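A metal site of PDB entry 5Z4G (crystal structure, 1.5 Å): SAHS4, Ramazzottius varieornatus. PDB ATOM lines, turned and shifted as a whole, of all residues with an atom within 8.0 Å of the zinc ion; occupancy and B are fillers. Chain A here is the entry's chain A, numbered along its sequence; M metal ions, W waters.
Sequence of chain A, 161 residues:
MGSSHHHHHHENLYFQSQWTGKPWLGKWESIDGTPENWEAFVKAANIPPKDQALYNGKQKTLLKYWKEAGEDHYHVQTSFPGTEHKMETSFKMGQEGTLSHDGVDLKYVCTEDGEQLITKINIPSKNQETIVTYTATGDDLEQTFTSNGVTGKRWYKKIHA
A ring nitrogen (NE2) of His 75 is bound to the zinc ion, 2.1 Å away. The zinc ion is bound by water W2. NE2 of His 73 binds the zinc ion, at 2.1 Å. The side-chain carboxylate (OE2) of Glu 68 is bound to the zinc ion (2.3 Å). The zinc ion is bound by water W1 (2.3 Å). OE2 of Glu 71 is bound to the zinc ion (2.3 Å). The zinc ion has six donor atoms within binding distance.
Of the 12 residues printed, 4 come within 4 Å of the zinc ion. The nearest printed residue that does not touch the zinc ion is Ser 90 (5.4 Å).
The backbone NH of His 75 is in hydrogen-bond range of the backbone carbonyl oxygen of Trp 66, at 2.8 Å.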
ATOM      1  N   TRP A  66      26.378 -14.418   2.524  1.00  0.00           N
ATOM      2  CA  TRP A  66      25.751 -14.486   1.196  1.00  0.00           C
ATOM      3  C   TRP A  66      24.524 -15.375   1.189  1.00  0.00           C
ATOM      4  O   TRP A  66      24.321 -16.200   2.100  1.00  0.00           O
ATOM      5  CB  TRP A  66      26.755 -14.865   0.103  1.00  0.00           C
ATOM      6  CG  TRP A  66      27.210 -16.308   0.038  1.00  0.00           C
ATOM      7  CD1 TRP A  66      26.766 -17.260  -0.850  1.00  0.00           C
ATOM      8  CD2 TRP A  66      28.246 -16.928   0.806  1.00  0.00           C
ATOM      9  NE1 TRP A  66      27.437 -18.444  -0.641  1.00  0.00           N
ATOM     10  CE2 TRP A  66      28.363 -18.270   0.362  1.00  0.00           C
ATOM     11  CE3 TRP A  66      29.063 -16.493   1.865  1.00  0.00           C
ATOM     12  CZ2 TRP A  66      29.268 -19.181   0.918  1.00  0.00           C
ATOM     13  CZ3 TRP A  66      29.977 -17.401   2.426  1.00  0.00           C
ATOM     14  CH2 TRP A  66      30.068 -18.722   1.947  1.00  0.00           C
ATOM     15  N   LYS A  67      23.688 -15.173   0.178  1.00  0.00           N
ATOM     16  CA  LYS A  67      22.481 -15.938  -0.031  1.00  0.00           C
ATOM     17  C   LYS A  67      22.410 -16.280  -1.505  1.00  0.00           C
ATOM     18  O   LYS A  67      22.462 -15.391  -2.354  1.00  0.00           O
ATOM     19  CB  LYS A  67      21.265 -15.111   0.394  1.00  0.00           C
ATOM     20  CG  LYS A  67      19.909 -15.755   0.124  1.00  0.00           C
ATOM     21  CD  LYS A  67      19.336 -16.424   1.357  1.00  0.00           C
ATOM     22  CE  LYS A  67      17.928 -16.933   1.105  1.00  0.00           C
ATOM     23  NZ  LYS A  67      17.097 -16.939   2.340  1.00  0.00           N
ATOM     24  N   GLU A  68      22.315 -17.565  -1.828  1.00  0.00           N
ATOM     25  CA  GLU A  68      22.019 -17.932  -3.218  1.00  0.00           C
ATOM     26  C   GLU A  68      20.517 -17.988  -3.477  1.00  0.00           C
ATOM     27  O   GLU A  68      19.755 -18.454  -2.622  1.00  0.00           O
ATOM     28  CB  GLU A  68      22.742 -19.195  -3.690  1.00  0.00           C
ATOM     29  CG  GLU A  68      22.558 -20.441  -2.853  1.00  0.00           C
ATOM     30  CD  GLU A  68      23.787 -20.807  -2.032  1.00  0.00           C
ATOM     31  OE1 GLU A  68      24.888 -20.282  -2.321  1.00  0.00           O
ATOM     32  OE2 GLU A  68      23.638 -21.625  -1.096  1.00  0.00           O
ATOM     33  N   GLY A  70      18.141 -19.634  -5.067  1.00  0.00           N
ATOM     34  CA  GLY A  70      17.273 -20.808  -4.936  1.00  0.00           C
ATOM     35  C   GLY A  70      17.372 -21.609  -3.653  1.00  0.00           C
ATOM     36  O   GLY A  70      16.873 -22.741  -3.604  1.00  0.00           O
ATOM     37  N   GLU A  71      18.000 -21.049  -2.618  1.00  0.00           N
ATOM     38  CA  GLU A  71      18.098 -21.711  -1.305  1.00  0.00           C
ATOM     39  C   GLU A  71      17.356 -20.923  -0.217  1.00  0.00           C
ATOM     40  O   GLU A  71      17.121 -19.732  -0.355  1.00  0.00           O
ATOM     41  CB  GLU A  71      19.556 -22.024  -0.919  1.00  0.00           C
ATOM     42  CG  GLU A  71      20.289 -22.908  -1.921  1.00  0.00           C
ATOM     43  CD  GLU A  71      21.036 -24.079  -1.291  1.00  0.00           C
ATOM     44  OE1 GLU A  71      20.388 -25.098  -0.971  1.00  0.00           O
ATOM     45  OE2 GLU A  71      22.272 -23.989  -1.124  1.00  0.00           O
ATOM     46  N   ASP A  72      16.978 -21.624   0.864  1.00  0.00           N
ATOM     47  CA  ASP A  72      16.220 -21.025   1.969  1.00  0.00           C
ATOM     48  C   ASP A  72      17.113 -20.717   3.175  1.00  0.00           C
ATOM     49  O   ASP A  72      16.628 -20.382   4.268  1.00  0.00           O
ATOM     50  CB  ASP A  72      15.064 -21.953   2.382  1.00  0.00           C
ATOM     51  CG  ASP A  72      15.548 -23.280   2.969  1.00  0.00           C
ATOM     52  OD1 ASP A  72      16.736 -23.636   2.778  1.00  0.00           O
ATOM     53  OD2 ASP A  72      14.748 -23.959   3.632  1.00  0.00           O
ATOM     54  N   HIS A  73      18.425 -20.834   2.972  1.00  0.00           N
ATOM     55  CA  HIS A  73      19.399 -20.567   4.029  1.00  0.00           C
ATOM     56  C   HIS A  73      20.418 -19.522   3.584  1.00  0.00           C
ATOM     57  O   HIS A  73      20.553 -19.253   2.385  1.00  0.00           O
ATOM     58  CB  HIS A  73      20.099 -21.858   4.474  1.00  0.00           C
ATOM     59  CG  HIS A  73      20.855 -22.540   3.380  1.00  0.00           C
ATOM     60  ND1 HIS A  73      20.360 -23.652   2.713  1.00  0.00           N
ATOM     61  CD2 HIS A  73      22.080 -22.297   2.844  1.00  0.00           C
ATOM     62  CE1 HIS A  73      21.245 -24.055   1.818  1.00  0.00           C
ATOM     63  NE2 HIS A  73      22.291 -23.248   1.875  1.00  0.00           N
ATOM     64  N   TYR A  74      21.097 -18.935   4.565  1.00  0.00           N
ATOM     65  CA  TYR A  74      22.215 -18.021   4.344  1.00  0.00           C
ATOM     66  C   TYR A  74      23.518 -18.733   4.620  1.00  0.00           C
ATOM     67  O   TYR A  74      23.546 -19.719   5.365  1.00  0.00           O
ATOM     68  CB  TYR A  74      22.112 -16.806   5.294  1.00  0.00           C
ATOM     69  CG  TYR A  74      20.949 -15.911   4.959  1.00  0.00           C
ATOM     70  CD1 TYR A  74      19.669 -16.163   5.447  1.00  0.00           C
ATOM     71  CD2 TYR A  74      21.132 -14.813   4.101  1.00  0.00           C
ATOM     72  CE1 TYR A  74      18.600 -15.351   5.091  1.00  0.00           C
ATOM     73  CE2 TYR A  74      20.074 -13.985   3.761  1.00  0.00           C
ATOM     74  CZ  TYR A  74      18.819 -14.261   4.262  1.00  0.00           C
ATOM     75  OH  TYR A  74      17.752 -13.455   3.929  1.00  0.00           O
ATOM     76  N   HIS A  75      24.598 -18.234   4.024  1.00  0.00           N
ATOM     77  CA  HIS A  75      25.945 -18.713   4.317  1.00  0.00           C
ATOM     78  C   HIS A  75      26.773 -17.640   4.985  1.00  0.00           C
ATOM     79  O   HIS A  75      26.614 -16.448   4.706  1.00  0.00           O
ATOM     80  CB  HIS A  75      26.634 -19.125   3.033  1.00  0.00           C
ATOM     81  CG  HIS A  75      26.192 -20.446   2.494  1.00  0.00           C
ATOM     82  ND1 HIS A  75      26.834 -21.626   2.788  1.00  0.00           N
ATOM     83  CD2 HIS A  75      25.159 -20.769   1.675  1.00  0.00           C
ATOM     84  CE1 HIS A  75      26.216 -22.626   2.184  1.00  0.00           C
ATOM     85  NE2 HIS A  75      25.194 -22.137   1.501  1.00  0.00           N
ATOM     86  N   THR A  89      29.730 -21.926   7.651  1.00  0.00           N
ATOM     87  CA  THR A  89      28.487 -22.597   7.976  1.00  0.00           C
ATOM     88  C   THR A  89      27.290 -21.974   7.232  1.00  0.00           C
ATOM     89  O   THR A  89      27.455 -21.024   6.467  1.00  0.00           O
ATOM     90  CB  THR A  89      28.259 -22.687   9.526  1.00  0.00           C
ATOM     91  OG1 THR A  89      27.309 -23.725   9.816  1.00  0.00           O
ATOM     92  CG2 THR A  89      27.796 -21.370  10.140  1.00  0.00           C
ATOM     93  N   SER A  90      26.128 -22.565   7.449  1.00  0.00           N
ATOM     94  CA  SER A  90      24.883 -22.064   6.895  1.00  0.00           C
ATOM     95  C   SER A  90      23.874 -21.951   8.034  1.00  0.00           C
ATOM     96  O   SER A  90      24.001 -22.636   9.052  1.00  0.00           O
ATOM     97  CB  SER A  90      24.365 -22.999   5.806  1.00  0.00           C
ATOM     98  OG  SER A  90      24.271 -24.324   6.279  1.00  0.00           O
ATOM     99  N   PHE A  91      22.902 -21.068   7.866  1.00  0.00           N
ATOM    100  CA  PHE A  91      21.870 -20.884   8.882  1.00  0.00           C
ATOM    101  C   PHE A  91      20.562 -20.440   8.255  1.00  0.00           C
ATOM    102  O   PHE A  91      20.533 -19.867   7.152  1.00  0.00           O
ATOM    103  CB  PHE A  91      22.335 -19.899   9.978  1.00  0.00           C
ATOM    104  CG  PHE A  91      22.598 -18.480   9.495  1.00  0.00           C
ATOM    105  CD1 PHE A  91      21.585 -17.513   9.483  1.00  0.00           C
ATOM    106  CD2 PHE A  91      23.874 -18.107   9.058  1.00  0.00           C
ATOM    107  CE1 PHE A  91      21.835 -16.218   9.040  1.00  0.00           C
ATOM    108  CE2 PHE A  91      24.119 -16.815   8.602  1.00  0.00           C
ATOM    109  CZ  PHE A  91      23.115 -15.864   8.605  1.00  0.00           C
HETATM  110 ZN    ZN M   1      23.870 -23.298   0.427  1.00  0.00          ZN
HETATM  111  O   HOH W   1      25.570 -23.821  -1.057  1.00  0.00           O
HETATM  112  O   HOH W   2      24.347 -25.148   1.317  1.00  0.00           O
